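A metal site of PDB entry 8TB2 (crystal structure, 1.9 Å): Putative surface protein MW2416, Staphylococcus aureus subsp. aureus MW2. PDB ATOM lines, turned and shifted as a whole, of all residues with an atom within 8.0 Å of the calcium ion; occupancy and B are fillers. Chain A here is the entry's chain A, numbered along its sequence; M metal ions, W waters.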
ATOM      1  N   VAL A  77      -6.975  23.381  13.215  1.00  0.00           N
ATOM      2  CA  VAL A  77      -8.001  24.409  13.035  1.00  0.00           C
ATOM      3  C   VAL A  77      -7.448  25.801  13.261  1.00  0.00           C
ATOM      4  O   VAL A  77      -8.033  26.794  12.800  1.00  0.00           O
ATOM      5  CB  VAL A  77      -9.193  24.087  13.967  1.00  0.00           C
ATOM      6  CG1 VAL A  77      -8.896  24.524  15.389  1.00  0.00           C
ATOM      7  CG2 VAL A  77     -10.461  24.702  13.441  1.00  0.00           C
ATOM      8  N   ALA A  81      -6.801  26.387   6.544  1.00  0.00           N
ATOM      9  CA  ALA A  81      -7.708  27.262   5.822  1.00  0.00           C
ATOM     10  C   ALA A  81      -8.962  27.563   6.644  1.00  0.00           C
ATOM     11  O   ALA A  81      -9.343  26.828   7.558  1.00  0.00           O
ATOM     12  CB  ALA A  81      -8.111  26.627   4.497  1.00  0.00           C
ATOM     13  N   ASP A  82      -9.616  28.680   6.287  1.00  0.00           N
ATOM     14  CA  ASP A  82     -10.879  29.068   6.914  1.00  0.00           C
ATOM     15  C   ASP A  82     -11.962  28.016   6.677  1.00  0.00           C
ATOM     16  O   ASP A  82     -12.813  27.817   7.546  1.00  0.00           O
ATOM     17  CB  ASP A  82     -11.392  30.399   6.363  1.00  0.00           C
ATOM     18  CG  ASP A  82     -10.428  31.547   6.575  1.00  0.00           C
ATOM     19  OD1 ASP A  82      -9.657  31.518   7.553  1.00  0.00           O
ATOM     20  OD2 ASP A  82     -10.468  32.509   5.773  1.00  0.00           O
ATOM     21  N   GLY A  83     -11.975  27.398   5.510  1.00  0.00           N
ATOM     22  CA  GLY A  83     -12.997  26.439   5.177  1.00  0.00           C
ATOM     23  C   GLY A  83     -13.412  26.550   3.724  1.00  0.00           C
ATOM     24  O   GLY A  83     -12.678  27.087   2.891  1.00  0.00           O
ATOM     25  N   ILE A 102     -18.776  33.939   3.154  1.00  0.00           N
ATOM     26  CA  ILE A 102     -19.538  33.478   4.307  1.00  0.00           C
ATOM     27  C   ILE A 102     -18.667  32.794   5.355  1.00  0.00           C
ATOM     28  O   ILE A 102     -19.189  32.246   6.324  1.00  0.00           O
ATOM     29  CB  ILE A 102     -20.700  32.557   3.871  1.00  0.00           C
ATOM     30  CG1 ILE A 102     -20.202  31.417   2.962  1.00  0.00           C
ATOM     31  CG2 ILE A 102     -21.772  33.380   3.180  1.00  0.00           C
ATOM     32  CD1 ILE A 102     -21.288  30.325   2.623  1.00  0.00           C
ATOM     33  N   LEU A 103     -17.343  32.845   5.203  1.00  0.00           N
ATOM     34  CA  LEU A 103     -16.462  32.114   6.110  1.00  0.00           C
ATOM     35  C   LEU A 103     -15.936  32.963   7.269  1.00  0.00           C
ATOM     36  O   LEU A 103     -15.265  32.426   8.150  1.00  0.00           O
ATOM     37  CB  LEU A 103     -15.283  31.539   5.325  1.00  0.00           C
ATOM     38  CG  LEU A 103     -15.626  30.327   4.443  1.00  0.00           C
ATOM     39  CD1 LEU A 103     -14.525  30.096   3.438  1.00  0.00           C
ATOM     40  CD2 LEU A 103     -15.842  29.070   5.316  1.00  0.00           C
ATOM     41  N   GLY A 104     -16.228  34.269   7.302  1.00  0.00           N
ATOM     42  CA  GLY A 104     -15.841  35.118   8.397  1.00  0.00           C
ATOM     43  C   GLY A 104     -17.021  35.879   8.959  1.00  0.00           C
ATOM     44  O   GLY A 104     -18.180  35.542   8.707  1.00  0.00           O
ATOM     45  N   PRO A 105     -16.752  36.925   9.749  1.00  0.00           N
ATOM     46  CA  PRO A 105     -17.861  37.668  10.352  1.00  0.00           C
ATOM     47  C   PRO A 105     -18.593  38.574   9.377  1.00  0.00           C
ATOM     48  O   PRO A 105     -19.736  38.959   9.659  1.00  0.00           O
ATOM     49  CB  PRO A 105     -17.168  38.492  11.455  1.00  0.00           C
ATOM     50  CG  PRO A 105     -15.780  38.717  10.914  1.00  0.00           C
ATOM     51  CD  PRO A 105     -15.438  37.480  10.119  1.00  0.00           C
ATOM     52  N   LYS A 115     -21.447  26.573   4.356  1.00  0.00           N
ATOM     53  CA  LYS A 115     -20.021  26.598   4.628  1.00  0.00           C
ATOM     54  C   LYS A 115     -19.597  25.346   5.388  1.00  0.00           C
ATOM     55  O   LYS A 115     -20.325  24.834   6.236  1.00  0.00           O
ATOM     56  CB  LYS A 115     -19.625  27.852   5.422  1.00  0.00           C
ATOM     57  CG  LYS A 115     -19.977  27.848   6.894  1.00  0.00           C
ATOM     58  CD  LYS A 115     -19.134  28.890   7.640  1.00  0.00           C
ATOM     59  CE  LYS A 115     -19.703  29.199   9.019  1.00  0.00           C
ATOM     60  NZ  LYS A 115     -18.808  30.134   9.801  1.00  0.00           N
ATOM     61  N   ILE A 116     -18.443  24.836   5.001  1.00  0.00           N
ATOM     62  CA  ILE A 116     -17.700  23.847   5.757  1.00  0.00           C
ATOM     63  C   ILE A 116     -16.602  24.646   6.442  1.00  0.00           C
ATOM     64  O   ILE A 116     -15.659  25.098   5.788  1.00  0.00           O
ATOM     65  CB  ILE A 116     -17.125  22.755   4.850  1.00  0.00           C
ATOM     66  CG1 ILE A 116     -18.248  21.995   4.125  1.00  0.00           C
ATOM     67  CG2 ILE A 116     -16.192  21.837   5.626  1.00  0.00           C
ATOM     68  CD1 ILE A 116     -17.785  21.187   2.927  1.00  0.00           C
ATOM     69  N   ASP A 117     -16.757  24.895   7.740  1.00  0.00           N
ATOM     70  CA  ASP A 117     -15.863  25.760   8.491  1.00  0.00           C
ATOM     71  C   ASP A 117     -14.764  24.912   9.124  1.00  0.00           C
ATOM     72  O   ASP A 117     -15.042  24.075   9.986  1.00  0.00           O
ATOM     73  CB  ASP A 117     -16.622  26.543   9.554  1.00  0.00           C
ATOM     74  CG  ASP A 117     -15.807  27.698  10.121  1.00  0.00           C
ATOM     75  OD1 ASP A 117     -14.619  27.471  10.477  1.00  0.00           O
ATOM     76  OD2 ASP A 117     -16.348  28.816  10.228  1.00  0.00           O
ATOM     77  N   THR A 118     -13.516  25.139   8.683  1.00  0.00           N
ATOM     78  CA  THR A 118     -12.376  24.345   9.133  1.00  0.00           C
ATOM     79  C   THR A 118     -11.345  25.174   9.893  1.00  0.00           C
ATOM     80  O   THR A 118     -10.270  24.642  10.223  1.00  0.00           O
ATOM     81  CB  THR A 118     -11.703  23.642   7.937  1.00  0.00           C
ATOM     82  OG1 THR A 118     -11.229  24.632   7.003  1.00  0.00           O
ATOM     83  CG2 THR A 118     -12.672  22.716   7.201  1.00  0.00           C
ATOM     84  N   GLY A 119     -11.622  26.438  10.187  1.00  0.00           N
ATOM     85  CA  GLY A 119     -10.629  27.301  10.807  1.00  0.00           C
ATOM     86  C   GLY A 119     -11.236  28.097  11.946  1.00  0.00           C
ATOM     87  O   GLY A 119     -12.428  28.407  11.942  1.00  0.00           O
ATOM     88  N   TYR A 120     -10.392  28.435  12.916  1.00  0.00           N
ATOM     89  CA  TYR A 120     -10.827  29.234  14.060  1.00  0.00           C
ATOM     90  C   TYR A 120     -10.420  30.687  13.863  1.00  0.00           C
ATOM     91  O   TYR A 120      -9.227  31.021  13.847  1.00  0.00           O
ATOM     92  CB  TYR A 120     -10.262  28.684  15.371  1.00  0.00           C
ATOM     93  CG  TYR A 120     -10.656  29.543  16.544  1.00  0.00           C
ATOM     94  CD1 TYR A 120     -11.974  29.584  16.978  1.00  0.00           C
ATOM     95  CD2 TYR A 120      -9.731  30.380  17.169  1.00  0.00           C
ATOM     96  CE1 TYR A 120     -12.352  30.377  18.033  1.00  0.00           C
ATOM     97  CE2 TYR A 120     -10.108  31.185  18.242  1.00  0.00           C
ATOM     98  CZ  TYR A 120     -11.429  31.176  18.661  1.00  0.00           C
ATOM     99  OH  TYR A 120     -11.857  31.956  19.710  1.00  0.00           O
ATOM    100  N   ASN A 121     -11.404  31.563  13.732  1.00  0.00           N
ATOM    101  CA  ASN A 121     -11.182  32.994  13.590  1.00  0.00           C
ATOM    102  C   ASN A 121     -11.744  33.645  14.847  1.00  0.00           C
ATOM    103  O   ASN A 121     -12.962  33.635  15.053  1.00  0.00           O
ATOM    104  CB  ASN A 121     -11.865  33.509  12.323  1.00  0.00           C
ATOM    105  CG  ASN A 121     -11.760  35.012  12.155  1.00  0.00           C
ATOM    106  OD1 ASN A 121     -11.171  35.702  12.998  1.00  0.00           O
ATOM    107  ND2 ASN A 121     -12.312  35.538  11.073  1.00  0.00           N
ATOM    108  N   PHE A 122     -10.859  34.235  15.667  1.00  0.00           N
ATOM    109  CA  PHE A 122     -11.295  34.828  16.924  1.00  0.00           C
ATOM    110  C   PHE A 122     -12.234  36.007  16.705  1.00  0.00           C
ATOM    111  O   PHE A 122     -12.920  36.416  17.645  1.00  0.00           O
ATOM    112  CB  PHE A 122     -10.089  35.278  17.762  1.00  0.00           C
ATOM    113  CG  PHE A 122      -9.490  36.591  17.311  1.00  0.00           C
ATOM    114  CD1 PHE A 122      -8.584  36.637  16.262  1.00  0.00           C
ATOM    115  CD2 PHE A 122      -9.815  37.773  17.949  1.00  0.00           C
ATOM    116  CE1 PHE A 122      -8.040  37.830  15.838  1.00  0.00           C
ATOM    117  CE2 PHE A 122      -9.278  38.978  17.529  1.00  0.00           C
ATOM    118  CZ  PHE A 122      -8.395  39.006  16.466  1.00  0.00           C
ATOM    119  N   ASP A 124     -14.817  35.938  14.650  1.00  0.00           N
ATOM    120  CA  ASP A 124     -16.116  35.480  14.163  1.00  0.00           C
ATOM    121  C   ASP A 124     -16.944  34.952  15.315  1.00  0.00           C
ATOM    122  O   ASP A 124     -16.607  33.887  15.871  1.00  0.00           O
ATOM    123  CB  ASP A 124     -15.935  34.404  13.094  1.00  0.00           C
ATOM    124  CG  ASP A 124     -17.264  33.969  12.466  1.00  0.00           C
ATOM    125  OD1 ASP A 124     -18.309  34.556  12.798  1.00  0.00           O
ATOM    126  OD2 ASP A 124     -17.237  33.036  11.630  1.00  0.00           O
ATOM    127  N   MET A 126     -19.527  33.320  15.332  1.00  0.00           N
ATOM    128  CA  MET A 126     -20.034  31.980  15.080  1.00  0.00           C
ATOM    129  C   MET A 126     -19.033  30.920  15.524  1.00  0.00           C
ATOM    130  O   MET A 126     -19.428  29.870  16.071  1.00  0.00           O
ATOM    131  CB  MET A 126     -20.371  31.824  13.589  1.00  0.00           C
ATOM    132  CG  MET A 126     -21.445  30.778  13.294  1.00  0.00           C
ATOM    133  SD  MET A 126     -21.698  30.619  11.523  1.00  0.00           S
ATOM    134  CE  MET A 126     -22.166  32.278  11.039  1.00  0.00           C
ATOM    135  N   ASP A 127     -17.732  31.154  15.317  1.00  0.00           N
ATOM    136  CA  ASP A 127     -16.744  30.190  15.783  1.00  0.00           C
ATOM    137  C   ASP A 127     -16.784  30.034  17.298  1.00  0.00           C
ATOM    138  O   ASP A 127     -16.510  28.947  17.823  1.00  0.00           O
ATOM    139  CB  ASP A 127     -15.327  30.598  15.330  1.00  0.00           C
ATOM    140  CG  ASP A 127     -15.065  30.286  13.860  1.00  0.00           C
ATOM    141  OD1 ASP A 127     -15.878  29.583  13.228  1.00  0.00           O
ATOM    142  OD2 ASP A 127     -14.040  30.753  13.333  1.00  0.00           O
ATOM    143  N   LYS A 128     -17.158  31.080  18.033  1.00  0.00           N
ATOM    144  CA  LYS A 128     -17.253  30.944  19.478  1.00  0.00           C
ATOM    145  C   LYS A 128     -18.508  30.150  19.865  1.00  0.00           C
ATOM    146  O   LYS A 128     -18.450  29.319  20.784  1.00  0.00           O
ATOM    147  CB  LYS A 128     -17.249  32.320  20.135  1.00  0.00           C
ATOM    148  CG  LYS A 128     -15.845  32.809  20.479  1.00  0.00           C
ATOM    149  CD  LYS A 128     -15.696  34.292  20.209  1.00  0.00           C
ATOM    150  CE  LYS A 128     -14.253  34.754  20.382  1.00  0.00           C
ATOM    151  N   GLU A 130     -19.794  27.759  18.309  1.00  0.00           N
ATOM    152  CA  GLU A 130     -19.593  26.362  17.956  1.00  0.00           C
ATOM    153  C   GLU A 130     -18.447  25.714  18.712  1.00  0.00           C
ATOM    154  O   GLU A 130     -18.151  24.541  18.469  1.00  0.00           O
ATOM    155  CB  GLU A 130     -19.358  26.233  16.453  1.00  0.00           C
ATOM    156  CG  GLU A 130     -20.555  26.644  15.635  1.00  0.00           C
ATOM    157  CD  GLU A 130     -21.647  25.606  15.684  1.00  0.00           C
ATOM    158  OE1 GLU A 130     -21.325  24.420  15.860  1.00  0.00           O
ATOM    159  OE2 GLU A 130     -22.825  25.980  15.552  1.00  0.00           O
ATOM    160  N   GLN A 132     -15.330  26.233  18.381  1.00  0.00           N
ATOM    161  CA  GLN A 132     -14.332  25.898  17.363  1.00  0.00           C
ATOM    162  C   GLN A 132     -12.901  26.003  17.897  1.00  0.00           C
ATOM    163  O   GLN A 132     -11.990  25.414  17.315  1.00  0.00           O
ATOM    164  CB  GLN A 132     -14.504  26.828  16.160  1.00  0.00           C
ATOM    165  CG  GLN A 132     -13.686  26.462  14.919  1.00  0.00           C
ATOM    166  CD  GLN A 132     -14.410  25.470  14.028  1.00  0.00           C
ATOM    167  OE1 GLN A 132     -15.084  24.564  14.516  1.00  0.00           O
ATOM    168  NE2 GLN A 132     -14.287  25.653  12.717  1.00  0.00           N
ATOM    169  N   GLY A 139     -14.361  20.781  13.061  1.00  0.00           N
ATOM    170  CA  GLY A 139     -14.957  21.930  12.398  1.00  0.00           C
ATOM    171  C   GLY A 139     -16.471  21.845  12.490  1.00  0.00           C
ATOM    172  O   GLY A 139     -17.006  21.121  13.328  1.00  0.00           O
ATOM    173  N   TYR A 140     -17.167  22.584  11.627  1.00  0.00           N
ATOM    174  CA  TYR A 140     -18.619  22.506  11.627  1.00  0.00           C
ATOM    175  C   TYR A 140     -19.142  22.958  10.271  1.00  0.00           C
ATOM    176  O   TYR A 140     -18.423  23.584   9.488  1.00  0.00           O
ATOM    177  CB  TYR A 140     -19.248  23.341  12.762  1.00  0.00           C
ATOM    178  CG  TYR A 140     -19.049  24.852  12.681  1.00  0.00           C
ATOM    179  CD1 TYR A 140     -17.895  25.452  13.193  1.00  0.00           C
ATOM    180  CD2 TYR A 140     -20.035  25.677  12.134  1.00  0.00           C
ATOM    181  CE1 TYR A 140     -17.736  26.832  13.151  1.00  0.00           C
ATOM    182  CE2 TYR A 140     -19.863  27.046  12.066  1.00  0.00           C
ATOM    183  CZ  TYR A 140     -18.708  27.622  12.579  1.00  0.00           C
ATOM    184  OH  TYR A 140     -18.550  28.973  12.513  1.00  0.00           O
HETATM  185 CA    CA M   1     -14.380  29.612  11.345  1.00  0.00          CA
HETATM  186  O   HOH W   1     -15.027  31.642  10.713  1.00  0.00           O
HETATM  187  O   HOH W   2     -13.328  29.966   9.485  1.00  0.00           O
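Three residues have an atom within 4 Å of the calcium ion: Asp 117, Gly 119 and Asp 127.
N of Gln 132 is in hydrogen-bond range of O of Asp 127, at 3.0 Å. The backbone NH of Asn 121 sits close to the side-chain carboxylate of Asp 127, at 2.8 Å. The side-chain carboxylate (OD1) of Asp 127 lies close to the side-chain hydroxyl (OH) of Tyr 140 (2.8 Å). O of Asp 117 lies within hydrogen-bond range of NE2 of Gln 132 (3.2 Å). The backbone NH (N) of Asp 117 lies within hydrogen-bond range of the backbone carbonyl oxygen (O) of Tyr 140, at 2.7 Å. The side-chain amino group of Lys 115 lies close to the side-chain carboxylate of Asp 117 (2.8 Å). O of Gly 119 sits close to NE2 of Gln 132 (3.4 Å). The backbone NH (N) of Gly 119 is in hydrogen-bond range of the backbone carbonyl oxygen (O) of Asp 82, at 3.2 Å.
Water W2 bridges the backbone carbonyl oxygen (O) of Asp 82 and the backbone carbonyl oxygen (O) of Leu 103. Water W1 bridges O of Leu 103 (2.7 Å) and OD2 of Asp 124 (2.8 Å).
The calcium ion is bound by water W2 (2.2 Å), water W1 (2.2 Å), the side-chain carboxylate (OD2) of Asp 127 (2.3 Å), the side-chain carboxylate (OD1) of Asp 117 (2.3 Å), the backbone carbonyl oxygen (O) of Gly 119 (2.4 Å), the side-chain carboxylate (OD2) of Asp 117 (2.4 Å) and the side-chain carboxylate (OD1) of Asp 127 (2.4 Å). The calcium ion has seven donor atoms within binding distance.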
